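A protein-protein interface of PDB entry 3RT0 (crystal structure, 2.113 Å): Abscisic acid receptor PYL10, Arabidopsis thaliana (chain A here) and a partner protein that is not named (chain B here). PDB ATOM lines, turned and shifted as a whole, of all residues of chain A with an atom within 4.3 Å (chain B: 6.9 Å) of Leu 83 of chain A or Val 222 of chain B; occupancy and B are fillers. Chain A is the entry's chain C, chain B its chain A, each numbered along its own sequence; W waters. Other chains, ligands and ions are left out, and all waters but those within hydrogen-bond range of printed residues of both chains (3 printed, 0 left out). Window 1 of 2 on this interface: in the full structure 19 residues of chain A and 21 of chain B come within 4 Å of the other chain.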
ATOM      1  N   PHE A  58     -11.449  18.412 -17.988  1.00  0.00           N
ATOM      2  CA  PHE A  58     -12.038  19.426 -17.122  1.00  0.00           C
ATOM      3  C   PHE A  58     -13.571  19.366 -17.001  1.00  0.00           C
ATOM      4  O   PHE A  58     -14.163  20.177 -16.296  1.00  0.00           O
ATOM      5  CB  PHE A  58     -11.587  20.825 -17.547  1.00  0.00           C
ATOM      6  CG  PHE A  58     -10.156  21.123 -17.196  1.00  0.00           C
ATOM      7  CD1 PHE A  58      -9.766  21.214 -15.869  1.00  0.00           C
ATOM      8  CD2 PHE A  58      -9.206  21.300 -18.184  1.00  0.00           C
ATOM      9  CE1 PHE A  58      -8.443  21.488 -15.534  1.00  0.00           C
ATOM     10  CE2 PHE A  58      -7.891  21.569 -17.860  1.00  0.00           C
ATOM     11  CZ  PHE A  58      -7.511  21.662 -16.532  1.00  0.00           C
ATOM     12  N   LEU A  79     -18.022  22.548 -15.492  1.00  0.00           N
ATOM     13  CA  LEU A  79     -16.590  22.336 -15.439  1.00  0.00           C
ATOM     14  C   LEU A  79     -16.138  22.041 -14.016  1.00  0.00           C
ATOM     15  O   LEU A  79     -16.789  22.437 -13.052  1.00  0.00           O
ATOM     16  CB  LEU A  79     -15.856  23.564 -15.984  1.00  0.00           C
ATOM     17  CG  LEU A  79     -16.190  23.982 -17.421  1.00  0.00           C
ATOM     18  CD1 LEU A  79     -15.635  25.351 -17.732  1.00  0.00           C
ATOM     19  CD2 LEU A  79     -15.644  22.958 -18.406  1.00  0.00           C
ATOM     20  N   LYS A  80     -15.021  21.339 -13.895  1.00  0.00           N
ATOM     21  CA  LYS A  80     -14.392  21.121 -12.596  1.00  0.00           C
ATOM     22  C   LYS A  80     -13.771  22.428 -12.090  1.00  0.00           C
ATOM     23  O   LYS A  80     -13.509  23.348 -12.876  1.00  0.00           O
ATOM     24  CB  LYS A  80     -13.349  20.003 -12.708  1.00  0.00           C
ATOM     25  CG  LYS A  80     -13.981  18.638 -13.005  1.00  0.00           C
ATOM     26  CD  LYS A  80     -12.959  17.554 -13.310  1.00  0.00           C
ATOM     27  CE  LYS A  80     -13.659  16.231 -13.648  1.00  0.00           C
ATOM     28  NZ  LYS A  80     -12.729  15.163 -14.133  1.00  0.00           N
ATOM     29  N   SER A  81     -13.537  22.521 -10.784  1.00  0.00           N
ATOM     30  CA  SER A  81     -13.038  23.769 -10.211  1.00  0.00           C
ATOM     31  C   SER A  81     -11.602  24.082 -10.642  1.00  0.00           C
ATOM     32  O   SER A  81     -10.849  23.189 -11.040  1.00  0.00           O
ATOM     33  CB  SER A  81     -13.157  23.769  -8.686  1.00  0.00           C
ATOM     34  OG  SER A  81     -12.103  23.037  -8.104  1.00  0.00           O
ATOM     35  N   GLY A  82     -11.251  25.365 -10.616  1.00  0.00           N
ATOM     36  CA  GLY A  82      -9.897  25.786 -10.927  1.00  0.00           C
ATOM     37  C   GLY A  82      -9.775  26.614 -12.189  1.00  0.00           C
ATOM     38  O   GLY A  82      -8.792  27.338 -12.364  1.00  0.00           O
ATOM     39  N   LEU A  83     -10.764  26.499 -13.073  1.00  0.00           N
ATOM     40  CA  LEU A  83     -10.777  27.267 -14.310  1.00  0.00           C
ATOM     41  C   LEU A  83     -11.406  28.628 -14.093  1.00  0.00           C
ATOM     42  O   LEU A  83     -12.154  28.823 -13.140  1.00  0.00           O
ATOM     43  CB  LEU A  83     -11.595  26.527 -15.359  1.00  0.00           C
ATOM     44  CG  LEU A  83     -10.807  25.713 -16.378  1.00  0.00           C
ATOM     45  CD1 LEU A  83      -9.431  25.376 -15.843  1.00  0.00           C
ATOM     46  CD2 LEU A  83     -11.586  24.459 -16.726  1.00  0.00           C
ATOM     47  N   PRO A  84     -11.133  29.575 -15.003  1.00  0.00           N
ATOM     48  CA  PRO A  84     -11.846  30.861 -14.962  1.00  0.00           C
ATOM     49  C   PRO A  84     -13.216  30.759 -15.640  1.00  0.00           C
ATOM     50  O   PRO A  84     -13.576  31.617 -16.449  1.00  0.00           O
ATOM     51  CB  PRO A  84     -10.930  31.789 -15.756  1.00  0.00           C
ATOM     52  CG  PRO A  84     -10.222  30.882 -16.729  1.00  0.00           C
ATOM     53  CD  PRO A  84     -10.143  29.510 -16.094  1.00  0.00           C
ATOM     54  N   ALA A  85     -13.960  29.708 -15.315  1.00  0.00           N
ATOM     55  CA  ALA A  85     -15.262  29.452 -15.919  1.00  0.00           C
ATOM     56  C   ALA A  85     -15.871  28.282 -15.163  1.00  0.00           C
ATOM     57  O   ALA A  85     -15.151  27.523 -14.539  1.00  0.00           O
ATOM     58  CB  ALA A  85     -15.103  29.106 -17.388  1.00  0.00           C
ATOM     59  N   PHE A 155      -3.846  30.946 -23.499  1.00  0.00           N
ATOM     60  CA  PHE A 155      -4.921  30.360 -22.724  1.00  0.00           C
ATOM     61  C   PHE A 155      -5.588  29.202 -23.491  1.00  0.00           C
ATOM     62  O   PHE A 155      -5.580  28.061 -23.035  1.00  0.00           O
ATOM     63  CB  PHE A 155      -5.927  31.457 -22.374  1.00  0.00           C
ATOM     64  CG  PHE A 155      -7.142  30.977 -21.621  1.00  0.00           C
ATOM     65  CD1 PHE A 155      -7.023  30.409 -20.364  1.00  0.00           C
ATOM     66  CD2 PHE A 155      -8.420  31.143 -22.161  1.00  0.00           C
ATOM     67  CE1 PHE A 155      -8.157  29.983 -19.657  1.00  0.00           C
ATOM     68  CE2 PHE A 155      -9.557  30.721 -21.469  1.00  0.00           C
ATOM     69  CZ  PHE A 155      -9.431  30.139 -20.223  1.00  0.00           C
ATOM     70  N   ALA A 158      -3.454  26.206 -24.173  1.00  0.00           N
ATOM     71  CA  ALA A 158      -3.254  25.460 -22.945  1.00  0.00           C
ATOM     72  C   ALA A 158      -4.407  24.482 -22.794  1.00  0.00           C
ATOM     73  O   ALA A 158      -4.190  23.300 -22.579  1.00  0.00           O
ATOM     74  CB  ALA A 158      -3.180  26.397 -21.737  1.00  0.00           C
ATOM     75  N   ARG B  28     -21.657  23.361  -5.499  1.00  0.00           N
ATOM     76  CA  ARG B  28     -20.849  22.860  -6.605  1.00  0.00           C
ATOM     77  C   ARG B  28     -21.410  21.573  -7.206  1.00  0.00           C
ATOM     78  O   ARG B  28     -22.162  20.850  -6.558  1.00  0.00           O
ATOM     79  CB  ARG B  28     -19.410  22.630  -6.150  1.00  0.00           C
ATOM     80  CG  ARG B  28     -18.508  23.832  -6.324  1.00  0.00           C
ATOM     81  CD  ARG B  28     -17.374  23.536  -7.287  1.00  0.00           C
ATOM     82  NE  ARG B  28     -17.301  24.526  -8.356  1.00  0.00           N
ATOM     83  CZ  ARG B  28     -16.955  24.248  -9.606  1.00  0.00           C
ATOM     84  NH1 ARG B  28     -16.917  25.212 -10.513  1.00  0.00           N
ATOM     85  NH2 ARG B  28     -16.643  23.007  -9.948  1.00  0.00           N
ATOM     86  N   HIS B  74      -8.335  20.909  -7.415  1.00  0.00           N
ATOM     87  CA  HIS B  74      -8.776  21.533  -8.657  1.00  0.00           C
ATOM     88  C   HIS B  74      -8.508  20.608  -9.812  1.00  0.00           C
ATOM     89  O   HIS B  74      -7.535  19.875  -9.805  1.00  0.00           O
ATOM     90  CB  HIS B  74      -8.119  22.896  -8.902  1.00  0.00           C
ATOM     91  CG  HIS B  74      -6.643  22.906  -8.665  1.00  0.00           C
ATOM     92  ND1 HIS B  74      -6.083  23.379  -7.495  1.00  0.00           N
ATOM     93  CD2 HIS B  74      -5.616  22.487  -9.433  1.00  0.00           C
ATOM     94  CE1 HIS B  74      -4.771  23.265  -7.563  1.00  0.00           C
ATOM     95  NE2 HIS B  74      -4.457  22.716  -8.724  1.00  0.00           N
ATOM     96  N   GLY B  75      -9.384  20.645 -10.810  1.00  0.00           N
ATOM     97  CA  GLY B  75      -9.239  19.778 -11.961  1.00  0.00           C
ATOM     98  C   GLY B  75      -9.663  18.354 -11.649  1.00  0.00           C
ATOM     99  O   GLY B  75      -9.447  17.455 -12.440  1.00  0.00           O
ATOM    100  N   ILE B 212      -1.236  35.660 -16.970  1.00  0.00           N
ATOM    101  CA  ILE B 212      -2.219  36.338 -17.788  1.00  0.00           C
ATOM    102  C   ILE B 212      -3.422  36.768 -16.974  1.00  0.00           C
ATOM    103  O   ILE B 212      -3.930  36.008 -16.161  1.00  0.00           O
ATOM    104  CB  ILE B 212      -2.697  35.426 -18.912  1.00  0.00           C
ATOM    105  CG1 ILE B 212      -1.506  34.987 -19.762  1.00  0.00           C
ATOM    106  CG2 ILE B 212      -3.741  36.132 -19.747  1.00  0.00           C
ATOM    107  CD1 ILE B 212      -1.847  33.900 -20.756  1.00  0.00           C
ATOM    108  N   TRP B 214      -7.007  37.093 -16.413  1.00  0.00           N
ATOM    109  CA  TRP B 214      -8.178  36.391 -16.913  1.00  0.00           C
ATOM    110  C   TRP B 214      -9.032  35.950 -15.733  1.00  0.00           C
ATOM    111  O   TRP B 214      -8.908  34.820 -15.253  1.00  0.00           O
ATOM    112  CB  TRP B 214      -7.741  35.163 -17.712  1.00  0.00           C
ATOM    113  CG  TRP B 214      -8.753  34.698 -18.708  1.00  0.00           C
ATOM    114  CD1 TRP B 214      -9.945  34.081 -18.448  1.00  0.00           C
ATOM    115  CD2 TRP B 214      -8.653  34.795 -20.133  1.00  0.00           C
ATOM    116  NE1 TRP B 214     -10.597  33.790 -19.626  1.00  0.00           N
ATOM    117  CE2 TRP B 214      -9.820  34.221 -20.674  1.00  0.00           C
ATOM    118  CE3 TRP B 214      -7.694  35.324 -21.005  1.00  0.00           C
ATOM    119  CZ2 TRP B 214     -10.055  34.166 -22.042  1.00  0.00           C
ATOM    120  CZ3 TRP B 214      -7.922  35.259 -22.372  1.00  0.00           C
ATOM    121  CH2 TRP B 214      -9.092  34.687 -22.874  1.00  0.00           C
ATOM    122  N   GLN B 215      -9.905  36.838 -15.281  1.00  0.00           N
ATOM    123  CA  GLN B 215     -10.649  36.623 -14.052  1.00  0.00           C
ATOM    124  C   GLN B 215      -9.635  36.422 -12.923  1.00  0.00           C
ATOM    125  O   GLN B 215      -9.675  35.429 -12.197  1.00  0.00           O
ATOM    126  CB  GLN B 215     -11.596  35.426 -14.188  1.00  0.00           C
ATOM    127  CG  GLN B 215     -12.686  35.358 -13.113  1.00  0.00           C
ATOM    128  CD  GLN B 215     -13.413  34.013 -13.083  1.00  0.00           C
ATOM    129  OE1 GLN B 215     -13.462  33.340 -12.043  1.00  0.00           O
ATOM    130  NE2 GLN B 215     -13.988  33.620 -14.222  1.00  0.00           N
ATOM    131  N   ARG B 218      -3.550  34.645 -13.671  1.00  0.00           N
ATOM    132  CA  ARG B 218      -3.541  33.194 -13.785  1.00  0.00           C
ATOM    133  C   ARG B 218      -2.340  32.689 -14.556  1.00  0.00           C
ATOM    134  O   ARG B 218      -1.898  33.309 -15.515  1.00  0.00           O
ATOM    135  CB  ARG B 218      -4.850  32.681 -14.423  1.00  0.00           C
ATOM    136  CG  ARG B 218      -6.082  32.779 -13.494  1.00  0.00           C
ATOM    137  CD  ARG B 218      -7.418  32.360 -14.163  1.00  0.00           C
ATOM    138  NE  ARG B 218      -8.543  32.609 -13.246  1.00  0.00           N
ATOM    139  CZ  ARG B 218      -9.165  31.679 -12.521  1.00  0.00           C
ATOM    140  NH1 ARG B 218      -8.837  30.388 -12.621  1.00  0.00           N
ATOM    141  NH2 ARG B 218     -10.149  32.040 -11.708  1.00  0.00           N
ATOM    142  N   VAL B 219      -1.815  31.546 -14.138  1.00  0.00           N
ATOM    143  CA  VAL B 219      -0.726  30.907 -14.869  1.00  0.00           C
ATOM    144  C   VAL B 219      -1.253  30.418 -16.234  1.00  0.00           C
ATOM    145  O   VAL B 219      -2.125  29.559 -16.292  1.00  0.00           O
ATOM    146  CB  VAL B 219      -0.150  29.733 -14.072  1.00  0.00           C
ATOM    147  CG1 VAL B 219       0.955  29.050 -14.857  1.00  0.00           C
ATOM    148  CG2 VAL B 219       0.383  30.226 -12.718  1.00  0.00           C
ATOM    149  N   PHE B 220      -0.727  30.977 -17.319  1.00  0.00           N
ATOM    150  CA  PHE B 220      -1.274  30.730 -18.664  1.00  0.00           C
ATOM    151  C   PHE B 220      -2.781  30.988 -18.779  1.00  0.00           C
ATOM    152  O   PHE B 220      -3.459  30.443 -19.663  1.00  0.00           O
ATOM    153  CB  PHE B 220      -0.915  29.329 -19.151  1.00  0.00           C
ATOM    154  CG  PHE B 220       0.491  29.219 -19.648  1.00  0.00           C
ATOM    155  CD1 PHE B 220       0.807  29.554 -20.961  1.00  0.00           C
ATOM    156  CD2 PHE B 220       1.507  28.815 -18.802  1.00  0.00           C
ATOM    157  CE1 PHE B 220       2.108  29.474 -21.423  1.00  0.00           C
ATOM    158  CE2 PHE B 220       2.815  28.726 -19.259  1.00  0.00           C
ATOM    159  CZ  PHE B 220       3.115  29.061 -20.572  1.00  0.00           C
ATOM    160  N   GLY B 221      -3.298  31.845 -17.901  1.00  0.00           N
ATOM    161  CA  GLY B 221      -4.712  32.182 -17.895  1.00  0.00           C
ATOM    162  C   GLY B 221      -5.592  31.122 -17.264  1.00  0.00           C
ATOM    163  O   GLY B 221      -6.791  31.326 -17.080  1.00  0.00           O
ATOM    164  N   VAL B 222      -4.985  30.002 -16.891  1.00  0.00           N
ATOM    165  CA  VAL B 222      -5.720  28.847 -16.375  1.00  0.00           C
ATOM    166  C   VAL B 222      -5.878  28.843 -14.853  1.00  0.00           C
ATOM    167  O   VAL B 222      -6.996  28.933 -14.342  1.00  0.00           O
ATOM    168  CB  VAL B 222      -5.015  27.541 -16.790  1.00  0.00           C
ATOM    169  CG1 VAL B 222      -5.750  26.321 -16.244  1.00  0.00           C
ATOM    170  CG2 VAL B 222      -4.883  27.477 -18.303  1.00  0.00           C
ATOM    171  N   LEU B 223      -4.753  28.723 -14.144  1.00  0.00           N
ATOM    172  CA  LEU B 223      -4.739  28.523 -12.692  1.00  0.00           C
ATOM    173  C   LEU B 223      -4.464  29.812 -11.919  1.00  0.00           C
ATOM    174  O   LEU B 223      -3.521  30.538 -12.231  1.00  0.00           O
ATOM    175  CB  LEU B 223      -3.686  27.467 -12.333  1.00  0.00           C
ATOM    176  CG  LEU B 223      -4.174  26.111 -11.814  1.00  0.00           C
ATOM    177  CD1 LEU B 223      -5.499  25.689 -12.433  1.00  0.00           C
ATOM    178  CD2 LEU B 223      -3.123  25.037 -11.993  1.00  0.00           C
ATOM    179  N   ALA B 224      -5.289  30.075 -10.907  1.00  0.00           N
ATOM    180  CA  ALA B 224      -5.212  31.293 -10.103  1.00  0.00           C
ATOM    181  C   ALA B 224      -4.185  31.200  -8.966  1.00  0.00           C
ATOM    182  O   ALA B 224      -3.930  32.181  -8.265  1.00  0.00           O
ATOM    183  CB  ALA B 224      -6.578  31.643  -9.536  1.00  0.00           C
ATOM    184  N   MET B 225      -3.584  30.029  -8.784  1.00  0.00           N
ATOM    185  CA  MET B 225      -2.510  29.877  -7.805  1.00  0.00           C
ATOM    186  C   MET B 225      -1.191  29.554  -8.508  1.00  0.00           C
ATOM    187  O   MET B 225      -1.191  28.974  -9.590  1.00  0.00           O
ATOM    188  CB  MET B 225      -2.855  28.817  -6.753  1.00  0.00           C
ATOM    189  CG  MET B 225      -2.814  27.385  -7.246  1.00  0.00           C
ATOM    190  SD  MET B 225      -4.227  26.962  -8.278  1.00  0.00           S
ATOM    191  CE  MET B 225      -5.571  27.133  -7.103  1.00  0.00           C
ATOM    192  N   TYR B 233       0.871  19.257 -15.759  1.00  0.00           N
ATOM    193  CA  TYR B 233       0.715  19.942 -17.048  1.00  0.00           C
ATOM    194  C   TYR B 233       1.274  21.365 -17.028  1.00  0.00           C
ATOM    195  O   TYR B 233       1.647  21.898 -18.068  1.00  0.00           O
ATOM    196  CB  TYR B 233      -0.730  19.942 -17.589  1.00  0.00           C
ATOM    197  CG  TYR B 233      -1.742  20.866 -16.916  1.00  0.00           C
ATOM    198  CD1 TYR B 233      -1.901  20.875 -15.531  1.00  0.00           C
ATOM    199  CD2 TYR B 233      -2.583  21.683 -17.673  1.00  0.00           C
ATOM    200  CE1 TYR B 233      -2.833  21.666 -14.927  1.00  0.00           C
ATOM    201  CE2 TYR B 233      -3.527  22.494 -17.069  1.00  0.00           C
ATOM    202  CZ  TYR B 233      -3.648  22.478 -15.692  1.00  0.00           C
ATOM    203  OH  TYR B 233      -4.580  23.266 -15.059  1.00  0.00           O
ATOM    204  N   LEU B 234       1.340  21.970 -15.845  1.00  0.00           N
ATOM    205  CA  LEU B 234       1.819  23.344 -15.728  1.00  0.00           C
ATOM    206  C   LEU B 234       3.145  23.480 -14.969  1.00  0.00           C
ATOM    207  O   LEU B 234       3.523  24.580 -14.566  1.00  0.00           O
ATOM    208  CB  LEU B 234       0.745  24.228 -15.096  1.00  0.00           C
ATOM    209  CG  LEU B 234      -0.487  24.467 -15.965  1.00  0.00           C
ATOM    210  CD1 LEU B 234      -1.538  25.208 -15.170  1.00  0.00           C
ATOM    211  CD2 LEU B 234      -0.111  25.229 -17.238  1.00  0.00           C
HETATM  212  O   HOH W   1     -12.930  32.043 -19.633  1.00  0.00           O
HETATM  213  O   HOH W   2     -10.725  29.766 -10.234  1.00  0.00           O
HETATM  214  O   HOH W   3      -7.287  28.146 -10.132  1.00  0.00           O
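The guanidinium group (NH2) of Arg 28 of chain B sits at hydrogen-bond distance from the backbone carbonyl oxygen (O) of Leu 79 of chain A (3.2 Å).
The backbone carbonyl oxygen (O) of Ser 81 of chain A is in hydrogen-bond range of the backbone NH (N) of Gly 75 of chain B (2.9 Å).
The side-chain amide nitrogen of Gln 215 of chain B sits at hydrogen-bond distance from the backbone carbonyl oxygen of Pro 84 of chain A (3.0 Å).
The guanidinium group (NH1) of Arg 218 of chain B sits at hydrogen-bond distance from the backbone carbonyl oxygen (O) of Gly 82 of chain A (3.1 Å).
NH2 of Arg 28 of chain B lies close to N of Ser 81 of chain A.
The backbone carbonyl oxygen of Val 222 of chain B sits close to the backbone carbonyl oxygen of Gly 82 of chain A.
The backbone nitrogen (N) of Pro 84 of chain A lies close to the guanidinium group (NH1) of Arg 218 of chain B, 3.4 Å away.
O of Arg 218 of chain B is in hydrogen-bond range of N of Ile 212 of chain B (2.8 Å).
The guanidinium group of Arg 218 of chain B is in hydrogen-bond range of the backbone carbonyl oxygen of Trp 214 of chain B (3.0 Å).
The backbone carbonyl oxygen (O) of Gln 215 of chain B lies within hydrogen-bond range of the guanidinium group (NE) of Arg 218 of chain B, 3.2 Å away.
The guanidinium group of Arg 218 of chain B is in hydrogen-bond range of the backbone carbonyl oxygen of Val 222 of chain B (2.9 Å).
The backbone carbonyl oxygen of Phe 58 of chain A lies within hydrogen-bond range of the backbone NH of Lys 80 of chain A, 2.8 Å away.
Lys 80 of chain A touches Arg 28 of chain B (C to NH2, 3.6 Å).
Lys 80 of chain A touches Gly 75 of chain B (CD to O, 3.6 Å).
Ser 81 of chain A touches His 74 of chain B (O to CB, 3.5 Å).
Gly 82 of chain A touches His 74 of chain B (CA to CB, 3.95 Å).
Leu 223 of chain B touches Gly 82 of chain A.
NH1 of Arg 218 of chain B touches C of Leu 83 of chain A, at 3.4 Å.
Val 222 of chain B touches Leu 83 of chain A.
Pro 84 of chain A touches Trp 214 of chain B (CG to CD1, 3.6 Å).
CD of Pro 84 of chain A touches O of Val 222 of chain B, at 3.6 Å.
CE1 of Phe 155 of chain A touches O of Gly 221 of chain B, 3.2 Å away.
Leu 83 of chain A touches just these residues of chain B: Arg 218 and Val 222.
Printed residues of chain A within 4 Å of Val 222 of chain B: Gly 82 (3.1 Å), Leu 83 (3.8 Å), Pro 84 (3.6 Å) and Ala 158 (3.98 Å).
Of chain B, only His 74 (3.95 Å), Arg 218 (3.1 Å), Val 222 (3.1 Å) and Leu 223 (3.7 Å) come within 4 Å of Gly 82 of chain A.
Of the printed residues of chain B, Lys 80 of chain A touches Arg 28 and Gly 75.
Of the printed residues of chain B, Leu 79 of chain A touches Arg 28 (3.2 Å).
Printed residues of chain A within 4 Å of Trp 214 of chain B: Pro 84 and Phe 155.
Of the printed residues of chain B, Phe 58 of chain A touches Tyr 233.
Of the printed residues of chain B, Ala 158 of chain A touches Val 222.
Ile 212 of chain B touches none of the printed residues of chain A.
The nearest residue of chain B that does not touch Leu 83 of chain A is Gln 215 of chain B (4.8 Å).
The nearest printed residue of chain A that does not touch Val 222 of chain B is Phe 155 of chain A (4.05 Å).
The nearest printed residue of chain A that does not touch Leu 223 of chain B is Leu 83 of chain A (5.2 Å).
Printed residues of chain A that touch a printed residue of chain B: Phe 58, Leu 79, Lys 80, Ser 81, Gly 82, Leu 83, Pro 84, Phe 155 and Ala 158.
Printed residues of chain B that touch a printed residue of chain A: Arg 28, His 74, Gly 75, Trp 214, Gln 215, Arg 218, Phe 220, Gly 221, Val 222, Leu 223 and Tyr 233.
Hydrophobic or aromatic side chains of chain B that line the printed part of chain A: His 74, Trp 214, Val 222, Leu 223 and Tyr 233.
Among the printed residues, 22 pairs touch across the chains.
Among the printed residues, no Asp or Glu carboxylate lies within 4 Å of a Lys or Arg side-chain nitrogen of the other chain.
Water W2 bridges NH2 of Arg 218 of chain B (2.8 Å) and O of Leu 83 of chain A (3.4 Å).
Water W3 lies within hydrogen-bond range of the backbone carbonyl oxygen (O) of Gly 82 of chain A, the backbone NH (N) of Ala 224 of chain B and the side-chain sulfur (SD) of Met 225 of chain B.
Water W1 bridges the indole nitrogen of Trp 214 of chain B and the backbone carbonyl oxygen of Pro 84 of chain A.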
